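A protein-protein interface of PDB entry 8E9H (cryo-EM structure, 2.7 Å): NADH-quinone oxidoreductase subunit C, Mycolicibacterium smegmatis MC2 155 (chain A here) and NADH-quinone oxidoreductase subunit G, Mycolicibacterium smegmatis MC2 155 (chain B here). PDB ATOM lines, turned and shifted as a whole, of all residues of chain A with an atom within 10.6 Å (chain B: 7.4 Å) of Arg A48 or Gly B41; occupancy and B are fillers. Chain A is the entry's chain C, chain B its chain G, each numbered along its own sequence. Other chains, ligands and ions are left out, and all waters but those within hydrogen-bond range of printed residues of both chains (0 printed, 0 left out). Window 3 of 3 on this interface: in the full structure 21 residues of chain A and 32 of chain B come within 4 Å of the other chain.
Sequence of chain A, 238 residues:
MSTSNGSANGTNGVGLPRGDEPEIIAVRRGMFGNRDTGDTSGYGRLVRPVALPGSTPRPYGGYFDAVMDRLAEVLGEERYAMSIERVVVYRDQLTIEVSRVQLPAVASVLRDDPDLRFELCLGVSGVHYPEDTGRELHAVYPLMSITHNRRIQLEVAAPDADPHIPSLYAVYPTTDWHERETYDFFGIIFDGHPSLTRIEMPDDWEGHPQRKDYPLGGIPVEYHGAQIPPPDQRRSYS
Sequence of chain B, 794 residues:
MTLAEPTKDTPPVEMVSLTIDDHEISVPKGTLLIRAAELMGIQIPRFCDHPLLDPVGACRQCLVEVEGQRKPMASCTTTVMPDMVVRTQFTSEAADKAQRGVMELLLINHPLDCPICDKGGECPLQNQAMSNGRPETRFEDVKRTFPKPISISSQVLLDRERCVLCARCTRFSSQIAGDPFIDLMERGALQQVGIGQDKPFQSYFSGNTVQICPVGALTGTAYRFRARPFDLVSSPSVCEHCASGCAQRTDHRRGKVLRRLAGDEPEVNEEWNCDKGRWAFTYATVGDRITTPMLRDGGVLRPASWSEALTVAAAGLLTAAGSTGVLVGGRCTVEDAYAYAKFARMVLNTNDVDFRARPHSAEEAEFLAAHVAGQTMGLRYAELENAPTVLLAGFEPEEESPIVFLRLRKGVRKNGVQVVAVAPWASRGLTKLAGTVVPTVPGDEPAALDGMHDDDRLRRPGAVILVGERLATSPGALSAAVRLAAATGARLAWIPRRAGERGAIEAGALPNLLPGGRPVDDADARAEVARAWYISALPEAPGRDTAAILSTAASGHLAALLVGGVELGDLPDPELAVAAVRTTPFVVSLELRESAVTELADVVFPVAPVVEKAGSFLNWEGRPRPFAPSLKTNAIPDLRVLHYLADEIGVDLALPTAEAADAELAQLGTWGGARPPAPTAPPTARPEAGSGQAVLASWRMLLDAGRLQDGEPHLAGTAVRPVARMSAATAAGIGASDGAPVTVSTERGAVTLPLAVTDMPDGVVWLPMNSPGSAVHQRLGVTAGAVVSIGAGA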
ATOM      1  N   GLU A  23      32.515 -14.683  20.273  1.00  0.00           N
ATOM      2  CA  GLU A  23      31.913 -14.478  21.588  1.00  0.00           C
ATOM      3  C   GLU A  23      30.844 -15.536  21.820  1.00  0.00           C
ATOM      4  O   GLU A  23      29.744 -15.440  21.273  1.00  0.00           O
ATOM      5  CB  GLU A  23      31.323 -13.075  21.690  1.00  0.00           C
ATOM      6  N   ILE A  24      31.151 -16.549  22.628  1.00  0.00           N
ATOM      7  CA  ILE A  24      30.168 -17.595  22.889  1.00  0.00           C
ATOM      8  C   ILE A  24      29.126 -17.027  23.846  1.00  0.00           C
ATOM      9  O   ILE A  24      29.454 -16.578  24.947  1.00  0.00           O
ATOM     10  CB  ILE A  24      30.818 -18.870  23.442  1.00  0.00           C
ATOM     11  CG1 ILE A  24      31.191 -18.724  24.918  1.00  0.00           C
ATOM     12  CG2 ILE A  24      32.045 -19.227  22.621  1.00  0.00           C
ATOM     13  CD1 ILE A  24      31.919 -19.924  25.477  1.00  0.00           C
ATOM     14  N   ILE A  25      27.867 -17.017  23.411  1.00  0.00           N
ATOM     15  CA  ILE A  25      26.790 -16.463  24.219  1.00  0.00           C
ATOM     16  C   ILE A  25      25.952 -17.545  24.881  1.00  0.00           C
ATOM     17  O   ILE A  25      25.275 -17.267  25.880  1.00  0.00           O
ATOM     18  CB  ILE A  25      25.889 -15.557  23.364  1.00  0.00           C
ATOM     19  CG1 ILE A  25      25.361 -16.318  22.148  1.00  0.00           C
ATOM     20  CG2 ILE A  25      26.655 -14.329  22.916  1.00  0.00           C
ATOM     21  CD1 ILE A  25      24.205 -15.633  21.467  1.00  0.00           C
ATOM     22  N   ALA A  26      25.972 -18.765  24.355  1.00  0.00           N
ATOM     23  CA  ALA A  26      25.230 -19.865  24.944  1.00  0.00           C
ATOM     24  C   ALA A  26      25.809 -21.167  24.419  1.00  0.00           C
ATOM     25  O   ALA A  26      26.265 -21.248  23.276  1.00  0.00           O
ATOM     26  CB  ALA A  26      23.736 -19.774  24.625  1.00  0.00           C
ATOM     27  N   VAL A  27      25.780 -22.185  25.269  1.00  0.00           N
ATOM     28  CA  VAL A  27      26.238 -23.523  24.918  1.00  0.00           C
ATOM     29  C   VAL A  27      25.033 -24.442  24.967  1.00  0.00           C
ATOM     30  O   VAL A  27      24.481 -24.690  26.045  1.00  0.00           O
ATOM     31  CB  VAL A  27      27.340 -24.020  25.864  1.00  0.00           C
ATOM     32  CG1 VAL A  27      27.810 -25.397  25.441  1.00  0.00           C
ATOM     33  CG2 VAL A  27      28.495 -23.043  25.889  1.00  0.00           C
ATOM     34  N   ARG A  28      24.630 -24.949  23.811  1.00  0.00           N
ATOM     35  CA  ARG A  28      23.502 -25.859  23.720  1.00  0.00           C
ATOM     36  C   ARG A  28      24.007 -27.288  23.599  1.00  0.00           C
ATOM     37  O   ARG A  28      24.843 -27.593  22.745  1.00  0.00           O
ATOM     38  CB  ARG A  28      22.611 -25.514  22.528  1.00  0.00           C
ATOM     39  CG  ARG A  28      23.312 -25.581  21.191  1.00  0.00           C
ATOM     40  CD  ARG A  28      22.386 -25.143  20.079  1.00  0.00           C
ATOM     41  NE  ARG A  28      21.969 -23.755  20.240  1.00  0.00           N
ATOM     42  CZ  ARG A  28      21.100 -23.139  19.452  1.00  0.00           C
ATOM     43  NH1 ARG A  28      20.542 -23.755  18.421  1.00  0.00           N
ATOM     44  NH2 ARG A  28      20.782 -21.873  19.702  1.00  0.00           N
ATOM     45  N   ARG A  29      23.495 -28.157  24.462  1.00  0.00           N
ATOM     46  CA  ARG A  29      23.891 -29.553  24.499  1.00  0.00           C
ATOM     47  C   ARG A  29      22.776 -30.402  23.916  1.00  0.00           C
ATOM     48  O   ARG A  29      21.605 -30.226  24.260  1.00  0.00           O
ATOM     49  CB  ARG A  29      24.204 -30.005  25.929  1.00  0.00           C
ATOM     50  N   GLY A  30      23.145 -31.315  23.027  1.00  0.00           N
ATOM     51  CA  GLY A  30      22.187 -32.224  22.436  1.00  0.00           C
ATOM     52  C   GLY A  30      21.670 -31.760  21.095  1.00  0.00           C
ATOM     53  O   GLY A  30      21.526 -30.559  20.851  1.00  0.00           O
ATOM     54  N   MET A  31      21.388 -32.712  20.217  1.00  0.00           N
ATOM     55  CA  MET A  31      20.847 -32.400  18.908  1.00  0.00           C
ATOM     56  C   MET A  31      19.422 -31.880  19.028  1.00  0.00           C
ATOM     57  O   MET A  31      18.743 -32.071  20.039  1.00  0.00           O
ATOM     58  CB  MET A  31      20.869 -33.639  18.018  1.00  0.00           C
ATOM     59  CG  MET A  31      22.257 -34.116  17.661  1.00  0.00           C
ATOM     60  SD  MET A  31      22.232 -35.630  16.690  1.00  0.00           S
ATOM     61  CE  MET A  31      21.586 -35.048  15.130  1.00  0.00           C
ATOM     62  N   PHE A  32      18.971 -31.207  17.974  1.00  0.00           N
ATOM     63  CA  PHE A  32      17.596 -30.752  17.816  1.00  0.00           C
ATOM     64  C   PHE A  32      17.276 -29.548  18.688  1.00  0.00           C
ATOM     65  O   PHE A  32      16.099 -29.262  18.924  1.00  0.00           O
ATOM     66  CB  PHE A  32      16.609 -31.881  18.120  1.00  0.00           C
ATOM     67  CG  PHE A  32      16.947 -33.167  17.429  1.00  0.00           C
ATOM     68  CD1 PHE A  32      17.548 -33.161  16.187  1.00  0.00           C
ATOM     69  CD2 PHE A  32      16.685 -34.379  18.031  1.00  0.00           C
ATOM     70  CE1 PHE A  32      17.868 -34.336  15.557  1.00  0.00           C
ATOM     71  CE2 PHE A  32      17.003 -35.557  17.401  1.00  0.00           C
ATOM     72  CZ  PHE A  32      17.597 -35.535  16.165  1.00  0.00           C
ATOM     73  N   GLY A  33      18.287 -28.844  19.182  1.00  0.00           N
ATOM     74  CA  GLY A  33      18.066 -27.608  19.902  1.00  0.00           C
ATOM     75  C   GLY A  33      17.157 -27.774  21.097  1.00  0.00           C
ATOM     76  O   GLY A  33      16.235 -26.980  21.295  1.00  0.00           O
ATOM     77  N   ASN A  34      17.403 -28.799  21.900  1.00  0.00           N
ATOM     78  CA  ASN A  34      16.554 -29.120  23.036  1.00  0.00           C
ATOM     79  C   ASN A  34      17.269 -28.737  24.324  1.00  0.00           C
ATOM     80  O   ASN A  34      18.368 -29.230  24.598  1.00  0.00           O
ATOM     81  CB  ASN A  34      16.203 -30.604  23.032  1.00  0.00           C
ATOM     82  CG  ASN A  34      15.276 -30.980  24.154  1.00  0.00           C
ATOM     83  OD1 ASN A  34      14.881 -30.140  24.960  1.00  0.00           O
ATOM     84  ND2 ASN A  34      14.913 -32.248  24.207  1.00  0.00           N
ATOM     85  N   ARG A  35      16.643 -27.861  25.110  1.00  0.00           N
ATOM     86  CA  ARG A  35      17.238 -27.431  26.371  1.00  0.00           C
ATOM     87  C   ARG A  35      17.148 -28.529  27.423  1.00  0.00           C
ATOM     88  O   ARG A  35      18.031 -28.661  28.278  1.00  0.00           O
ATOM     89  CB  ARG A  35      16.550 -26.159  26.860  1.00  0.00           C
ATOM     90  N   TYR A  43      20.579 -38.753  21.706  1.00  0.00           N
ATOM     91  CA  TYR A  43      20.879 -37.577  20.901  1.00  0.00           C
ATOM     92  C   TYR A  43      21.345 -36.392  21.731  1.00  0.00           C
ATOM     93  O   TYR A  43      21.596 -35.324  21.167  1.00  0.00           O
ATOM     94  CB  TYR A  43      19.652 -37.167  20.092  1.00  0.00           C
ATOM     95  CG  TYR A  43      19.335 -38.116  18.975  1.00  0.00           C
ATOM     96  CD1 TYR A  43      19.908 -37.968  17.728  1.00  0.00           C
ATOM     97  CD2 TYR A  43      18.449 -39.154  19.166  1.00  0.00           C
ATOM     98  CE1 TYR A  43      19.617 -38.837  16.708  1.00  0.00           C
ATOM     99  CE2 TYR A  43      18.150 -40.017  18.157  1.00  0.00           C
ATOM    100  CZ  TYR A  43      18.736 -39.860  16.927  1.00  0.00           C
ATOM    101  OH  TYR A  43      18.439 -40.731  15.911  1.00  0.00           O
ATOM    102  N   GLY A  44      21.464 -36.548  23.041  1.00  0.00           N
ATOM    103  CA  GLY A  44      21.776 -35.430  23.904  1.00  0.00           C
ATOM    104  C   GLY A  44      23.240 -35.164  24.138  1.00  0.00           C
ATOM    105  O   GLY A  44      23.572 -34.328  24.982  1.00  0.00           O
ATOM    106  N   ARG A  45      24.136 -35.839  23.427  1.00  0.00           N
ATOM    107  CA  ARG A  45      25.558 -35.729  23.712  1.00  0.00           C
ATOM    108  C   ARG A  45      26.264 -34.674  22.875  1.00  0.00           C
ATOM    109  O   ARG A  45      27.408 -34.330  23.186  1.00  0.00           O
ATOM    110  CB  ARG A  45      26.237 -37.081  23.500  1.00  0.00           C
ATOM    111  CG  ARG A  45      27.575 -37.201  24.191  1.00  0.00           C
ATOM    112  CD  ARG A  45      27.937 -38.649  24.426  1.00  0.00           C
ATOM    113  NE  ARG A  45      27.088 -39.261  25.440  1.00  0.00           N
ATOM    114  CZ  ARG A  45      27.380 -40.384  26.078  1.00  0.00           C
ATOM    115  NH1 ARG A  45      28.500 -41.046  25.837  1.00  0.00           N
ATOM    116  NH2 ARG A  45      26.527 -40.858  26.980  1.00  0.00           N
ATOM    117  N   LEU A  46      25.628 -34.154  21.830  1.00  0.00           N
ATOM    118  CA  LEU A  46      26.249 -33.104  21.036  1.00  0.00           C
ATOM    119  C   LEU A  46      26.425 -31.850  21.878  1.00  0.00           C
ATOM    120  O   LEU A  46      25.530 -31.466  22.633  1.00  0.00           O
ATOM    121  CB  LEU A  46      25.397 -32.793  19.808  1.00  0.00           C
ATOM    122  CG  LEU A  46      25.814 -31.569  18.994  1.00  0.00           C
ATOM    123  CD1 LEU A  46      27.163 -31.797  18.354  1.00  0.00           C
ATOM    124  CD2 LEU A  46      24.775 -31.255  17.940  1.00  0.00           C
ATOM    125  N   VAL A  47      27.583 -31.212  21.747  1.00  0.00           N
ATOM    126  CA  VAL A  47      27.877 -29.958  22.430  1.00  0.00           C
ATOM    127  C   VAL A  47      28.311 -28.959  21.373  1.00  0.00           C
ATOM    128  O   VAL A  47      29.394 -29.094  20.790  1.00  0.00           O
ATOM    129  CB  VAL A  47      28.957 -30.126  23.504  1.00  0.00           C
ATOM    130  CG1 VAL A  47      29.235 -28.799  24.177  1.00  0.00           C
ATOM    131  CG2 VAL A  47      28.526 -31.160  24.527  1.00  0.00           C
ATOM    132  N   ARG A  48      27.480 -27.953  21.130  1.00  0.00           N
ATOM    133  CA  ARG A  48      27.759 -26.928  20.128  1.00  0.00           C
ATOM    134  C   ARG A  48      27.664 -25.557  20.781  1.00  0.00           C
ATOM    135  O   ARG A  48      26.551 -25.135  21.158  1.00  0.00           O
ATOM    136  CB  ARG A  48      26.788 -27.024  18.958  1.00  0.00           C
ATOM    137  CG  ARG A  48      27.148 -26.112  17.796  1.00  0.00           C
ATOM    138  CD  ARG A  48      26.439 -26.524  16.522  1.00  0.00           C
ATOM    139  NE  ARG A  48      25.047 -26.087  16.521  1.00  0.00           N
ATOM    140  CZ  ARG A  48      24.025 -26.818  16.945  1.00  0.00           C
ATOM    141  NH1 ARG A  48      24.198 -28.035  17.434  1.00  0.00           N
ATOM    142  NH2 ARG A  48      22.797 -26.313  16.882  1.00  0.00           N
ATOM    143  N   PRO A  49      28.769 -24.832  20.939  1.00  0.00           N
ATOM    144  CA  PRO A  49      28.675 -23.475  21.488  1.00  0.00           C
ATOM    145  C   PRO A  49      28.098 -22.514  20.460  1.00  0.00           C
ATOM    146  O   PRO A  49      28.473 -22.541  19.286  1.00  0.00           O
ATOM    147  CB  PRO A  49      30.125 -23.131  21.837  1.00  0.00           C
ATOM    148  CG  PRO A  49      30.929 -23.943  20.900  1.00  0.00           C
ATOM    149  CD  PRO A  49      30.163 -25.209  20.652  1.00  0.00           C
ATOM    150  N   VAL A  50      27.184 -21.661  20.912  1.00  0.00           N
ATOM    151  CA  VAL A  50      26.550 -20.667  20.056  1.00  0.00           C
ATOM    152  C   VAL A  50      27.401 -19.406  20.139  1.00  0.00           C
ATOM    153  O   VAL A  50      27.299 -18.637  21.092  1.00  0.00           O
ATOM    154  CB  VAL A  50      25.106 -20.397  20.473  1.00  0.00           C
ATOM    155  CG1 VAL A  50      24.456 -19.417  19.516  1.00  0.00           C
ATOM    156  CG2 VAL A  50      24.323 -21.692  20.533  1.00  0.00           C
ATOM    157  N   ALA A  51      28.228 -19.183  19.126  1.00  0.00           N
ATOM    158  CA  ALA A  51      29.196 -18.097  19.139  1.00  0.00           C
ATOM    159  C   ALA A  51      28.785 -17.002  18.166  1.00  0.00           C
ATOM    160  O   ALA A  51      28.624 -17.255  16.969  1.00  0.00           O
ATOM    161  CB  ALA A  51      30.588 -18.618  18.786  1.00  0.00           C
ATOM    162  N   LEU A  52      28.611 -15.792  18.689  1.00  0.00           N
ATOM    163  CA  LEU A  52      28.472 -14.629  17.837  1.00  0.00           C
ATOM    164  C   LEU A  52      29.810 -14.320  17.166  1.00  0.00           C
ATOM    165  O   LEU A  52      30.875 -14.522  17.763  1.00  0.00           O
ATOM    166  CB  LEU A  52      28.013 -13.421  18.646  1.00  0.00           C
ATOM    167  CG  LEU A  52      26.560 -13.416  19.118  1.00  0.00           C
ATOM    168  CD1 LEU A  52      26.268 -12.134  19.874  1.00  0.00           C
ATOM    169  CD2 LEU A  52      25.601 -13.578  17.954  1.00  0.00           C
ATOM    170  N   GLU A 131      24.499 -16.285  29.625  1.00  0.00           N
ATOM    171  CA  GLU A 131      25.598 -17.237  29.572  1.00  0.00           C
ATOM    172  C   GLU A 131      26.925 -16.594  29.196  1.00  0.00           C
ATOM    173  O   GLU A 131      27.956 -17.272  29.239  1.00  0.00           O
ATOM    174  CB  GLU A 131      25.274 -18.354  28.576  1.00  0.00           C
ATOM    175  N   TYR A 237      12.056 -25.771  21.440  1.00  0.00           N
ATOM    176  CA  TYR A 237      13.225 -26.379  20.820  1.00  0.00           C
ATOM    177  C   TYR A 237      14.076 -25.328  20.132  1.00  0.00           C
ATOM    178  O   TYR A 237      14.517 -25.505  18.995  1.00  0.00           O
ATOM    179  CB  TYR A 237      12.808 -27.464  19.834  1.00  0.00           C
ATOM    180  CG  TYR A 237      12.134 -28.629  20.503  1.00  0.00           C
ATOM    181  CD1 TYR A 237      12.870 -29.700  20.979  1.00  0.00           C
ATOM    182  CD2 TYR A 237      10.762 -28.650  20.672  1.00  0.00           C
ATOM    183  CE1 TYR A 237      12.255 -30.761  21.597  1.00  0.00           C
ATOM    184  CE2 TYR A 237      10.140 -29.706  21.288  1.00  0.00           C
ATOM    185  CZ  TYR A 237      10.889 -30.760  21.747  1.00  0.00           C
ATOM    186  OH  TYR A 237      10.270 -31.816  22.365  1.00  0.00           O
ATOM    187  N   SER A 238      14.322 -24.217  20.814  1.00  0.00           N
ATOM    188  CA  SER A 238      15.161 -23.161  20.268  1.00  0.00           C
ATOM    189  C   SER A 238      16.597 -23.647  20.106  1.00  0.00           C
ATOM    190  O   SER A 238      16.900 -24.432  19.208  1.00  0.00           O
ATOM    191  CB  SER A 238      15.121 -21.926  21.169  1.00  0.00           C
ATOM    192  N   ILE B  25      41.401 -31.956  16.996  1.00  0.00           N
ATOM    193  CA  ILE B  25      40.877 -32.268  18.316  1.00  0.00           C
ATOM    194  C   ILE B  25      41.557 -33.523  18.835  1.00  0.00           C
ATOM    195  O   ILE B  25      41.924 -34.423  18.079  1.00  0.00           O
ATOM    196  CB  ILE B  25      39.348 -32.471  18.311  1.00  0.00           C
ATOM    197  CG1 ILE B  25      38.826 -32.602  19.741  1.00  0.00           C
ATOM    198  CG2 ILE B  25      38.978 -33.701  17.498  1.00  0.00           C
ATOM    199  CD1 ILE B  25      37.325 -32.486  19.849  1.00  0.00           C
ATOM    200  N   ARG B  35      31.307 -39.584  18.105  1.00  0.00           N
ATOM    201  CA  ARG B  35      31.476 -38.972  19.418  1.00  0.00           C
ATOM    202  C   ARG B  35      32.456 -37.809  19.363  1.00  0.00           C
ATOM    203  O   ARG B  35      32.235 -36.771  19.999  1.00  0.00           O
ATOM    204  CB  ARG B  35      31.948 -40.020  20.419  1.00  0.00           C
ATOM    205  CG  ARG B  35      31.031 -41.216  20.519  1.00  0.00           C
ATOM    206  CD  ARG B  35      29.773 -40.882  21.280  1.00  0.00           C
ATOM    207  NE  ARG B  35      28.712 -41.838  20.990  1.00  0.00           N
ATOM    208  CZ  ARG B  35      27.687 -41.603  20.182  1.00  0.00           C
ATOM    209  NH1 ARG B  35      27.529 -40.437  19.581  1.00  0.00           N
ATOM    210  NH2 ARG B  35      26.795 -42.564  19.972  1.00  0.00           N
ATOM    211  N   ALA B  36      33.551 -37.965  18.620  1.00  0.00           N
ATOM    212  CA  ALA B  36      34.494 -36.865  18.476  1.00  0.00           C
ATOM    213  C   ALA B  36      33.832 -35.666  17.818  1.00  0.00           C
ATOM    214  O   ALA B  36      34.020 -34.525  18.252  1.00  0.00           O
ATOM    215  CB  ALA B  36      35.707 -37.318  17.668  1.00  0.00           C
ATOM    216  N   ALA B  37      33.046 -35.906  16.771  1.00  0.00           N
ATOM    217  CA  ALA B  37      32.336 -34.813  16.120  1.00  0.00           C
ATOM    218  C   ALA B  37      31.374 -34.143  17.087  1.00  0.00           C
ATOM    219  O   ALA B  37      31.254 -32.913  17.104  1.00  0.00           O
ATOM    220  CB  ALA B  37      31.591 -35.330  14.893  1.00  0.00           C
ATOM    221  N   GLU B  38      30.676 -34.934  17.900  1.00  0.00           N
ATOM    222  CA  GLU B  38      29.797 -34.361  18.911  1.00  0.00           C
ATOM    223  C   GLU B  38      30.575 -33.439  19.838  1.00  0.00           C
ATOM    224  O   GLU B  38      30.169 -32.301  20.093  1.00  0.00           O
ATOM    225  CB  GLU B  38      29.125 -35.474  19.710  1.00  0.00           C
ATOM    226  CG  GLU B  38      28.031 -36.201  18.966  1.00  0.00           C
ATOM    227  CD  GLU B  38      27.559 -37.430  19.708  1.00  0.00           C
ATOM    228  OE1 GLU B  38      28.197 -37.798  20.714  1.00  0.00           O
ATOM    229  OE2 GLU B  38      26.552 -38.031  19.287  1.00  0.00           O
ATOM    230  N   LEU B  39      31.707 -33.921  20.351  1.00  0.00           N
ATOM    231  CA  LEU B  39      32.505 -33.099  21.251  1.00  0.00           C
ATOM    232  C   LEU B  39      32.984 -31.832  20.561  1.00  0.00           C
ATOM    233  O   LEU B  39      33.102 -30.783  21.200  1.00  0.00           O
ATOM    234  CB  LEU B  39      33.698 -33.893  21.777  1.00  0.00           C
ATOM    235  CG  LEU B  39      33.357 -35.063  22.695  1.00  0.00           C
ATOM    236  CD1 LEU B  39      34.616 -35.811  23.082  1.00  0.00           C
ATOM    237  CD2 LEU B  39      32.617 -34.587  23.929  1.00  0.00           C
ATOM    238  N   MET B  40      33.263 -31.908  19.265  1.00  0.00           N
ATOM    239  CA  MET B  40      33.706 -30.746  18.511  1.00  0.00           C
ATOM    240  C   MET B  40      32.554 -29.852  18.074  1.00  0.00           C
ATOM    241  O   MET B  40      32.795 -28.701  17.696  1.00  0.00           O
ATOM    242  CB  MET B  40      34.494 -31.194  17.280  1.00  0.00           C
ATOM    243  CG  MET B  40      35.105 -30.054  16.490  1.00  0.00           C
ATOM    244  SD  MET B  40      36.029 -30.624  15.059  1.00  0.00           S
ATOM    245  CE  MET B  40      37.457 -31.343  15.843  1.00  0.00           C
ATOM    246  N   GLY B  41      31.319 -30.339  18.122  1.00  0.00           N
ATOM    247  CA  GLY B  41      30.176 -29.535  17.749  1.00  0.00           C
ATOM    248  C   GLY B  41      29.663 -29.741  16.343  1.00  0.00           C
ATOM    249  O   GLY B  41      28.810 -28.968  15.896  1.00  0.00           O
ATOM    250  N   ILE B  42      30.151 -30.751  15.630  1.00  0.00           N
ATOM    251  CA  ILE B  42      29.663 -31.083  14.297  1.00  0.00           C
ATOM    252  C   ILE B  42      28.498 -32.048  14.444  1.00  0.00           C
ATOM    253  O   ILE B  42      28.599 -33.055  15.153  1.00  0.00           O
ATOM    254  CB  ILE B  42      30.769 -31.686  13.418  1.00  0.00           C
ATOM    255  CG1 ILE B  42      31.886 -30.672  13.194  1.00  0.00           C
ATOM    256  CG2 ILE B  42      30.205 -32.141  12.090  1.00  0.00           C
ATOM    257  CD1 ILE B  42      32.950 -30.705  14.229  1.00  0.00           C
ATOM    258  N   GLN B  43      27.395 -31.742  13.772  1.00  0.00           N
ATOM    259  CA  GLN B  43      26.172 -32.530  13.874  1.00  0.00           C
ATOM    260  C   GLN B  43      26.118 -33.498  12.702  1.00  0.00           C
ATOM    261  O   GLN B  43      25.688 -33.156  11.601  1.00  0.00           O
ATOM    262  CB  GLN B  43      24.955 -31.616  13.897  1.00  0.00           C
ATOM    263  CG  GLN B  43      23.656 -32.336  14.146  1.00  0.00           C
ATOM    264  CD  GLN B  43      22.499 -31.387  14.351  1.00  0.00           C
ATOM    265  OE1 GLN B  43      22.570 -30.473  15.172  1.00  0.00           O
ATOM    266  NE2 GLN B  43      21.424 -31.595  13.604  1.00  0.00           N
ATOM    267  N   ILE B  44      26.569 -34.720  12.938  1.00  0.00           N
ATOM    268  CA  ILE B  44      26.500 -35.765  11.915  1.00  0.00           C
ATOM    269  C   ILE B  44      25.169 -36.498  12.056  1.00  0.00           C
ATOM    270  O   ILE B  44      24.866 -37.004  13.146  1.00  0.00           O
ATOM    271  CB  ILE B  44      27.670 -36.730  12.054  1.00  0.00           C
ATOM    272  CG1 ILE B  44      28.988 -35.994  11.825  1.00  0.00           C
ATOM    273  CG2 ILE B  44      27.529 -37.869  11.066  1.00  0.00           C
ATOM    274  CD1 ILE B  44      30.201 -36.771  12.256  1.00  0.00           C
ATOM    275  N   PHE B  90      29.645 -31.163   6.078  1.00  0.00           N
ATOM    276  CA  PHE B  90      29.895 -29.729   6.069  1.00  0.00           C
ATOM    277  C   PHE B  90      31.096 -29.359   5.217  1.00  0.00           C
ATOM    278  O   PHE B  90      31.182 -28.217   4.757  1.00  0.00           O
ATOM    279  CB  PHE B  90      30.102 -29.225   7.495  1.00  0.00           C
ATOM    280  CG  PHE B  90      28.877 -29.319   8.348  1.00  0.00           C
ATOM    281  CD1 PHE B  90      27.784 -28.512   8.102  1.00  0.00           C
ATOM    282  CD2 PHE B  90      28.817 -30.212   9.399  1.00  0.00           C
ATOM    283  CE1 PHE B  90      26.655 -28.596   8.885  1.00  0.00           C
ATOM    284  CE2 PHE B  90      27.691 -30.299  10.185  1.00  0.00           C
ATOM    285  CZ  PHE B  90      26.610 -29.491   9.929  1.00  0.00           C
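N of Val A47 lies within hydrogen-bond range of O of Glu B38 (3.3 Å).
Of chain B, only Gly B41 (3.5 Å) and Gln B43 (3.7 Å) come within 4 Å of Arg A48. Of chain A, only Leu A46 (3.8 Å), Val A47 (3.2 Å) and Arg A48 (3.5 Å) come within 4 Å of Gly B41. No residue of chain A comes within 4 Å of Ala B37. Of the printed residues of chain A, Glu B38 touches Arg A45 (3.5 Å), Leu A46 (3.5 Å) and Val A47 (3.3 Å). Of the printed residues of chain A, Gln B43 touches Met A31 (3.6 Å), Leu A46 (3.6 Å) and Arg A48 (3.7 Å). Of the printed residues of chain B, Val A47 touches Glu B38 and Gly B41. Of the printed residues of chain B, Leu A46 touches Glu B38, Gly B41, Ile B42 and Gln B43. Leu B39 touches none of the printed residues of chain A. The nearest residue of chain B that does not touch Arg A48 is Glu B38 (5.2 Å).
CE of Met A31 touches CG of Gln B43 (3.6 Å). OE1 of Glu B38 touches CB of Arg A45, 3.5 Å away. CD1 of Leu A46 touches O of Glu B38 (3.5 Å). CD1 of Leu A46 touches C of Gly B41, 3.8 Å away. Leu A46 touches Ile B42. CD2 of Leu A46 touches OE1 of Gln B43, at 3.6 Å. Val A47 touches Gly B41 (O to CA, 3.2 Å). Arg A48 touches Gly B41 (CD to O, 3.5 Å). NH1 of Arg A48 touches OE1 of Gln B43, at 3.7 Å.
Of the 12 printed residues of chain B, 4 touch a printed residue of chain A. Along chain B the printed residues that touch a printed residue of chain A span positions 38 to 43. Hydrophobic or aromatic side chains of chain A within 4 Å of the printed part of chain B: Met A31 and Leu A46. Among the printed residues, 10 pairs touch across the chains.
O of Arg A28 lies within hydrogen-bond range of N of Arg A48 (3.1 Å). N of Gly A30 sits at hydrogen-bond distance from O of Leu A46, 2.4 Å away. The backbone NH (N) of Met A31 is in hydrogen-bond range of the backbone carbonyl oxygen (O) of Tyr A43 (2.8 Å). The guanidinium group of Arg B35 lies within salt-bridge range of the side-chain carboxylate of Glu B38 (2.6 Å). The backbone carbonyl oxygen (O) of Ala B37 sits at hydrogen-bond distance from the backbone NH (N) of Ile B42, at 2.8 Å.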
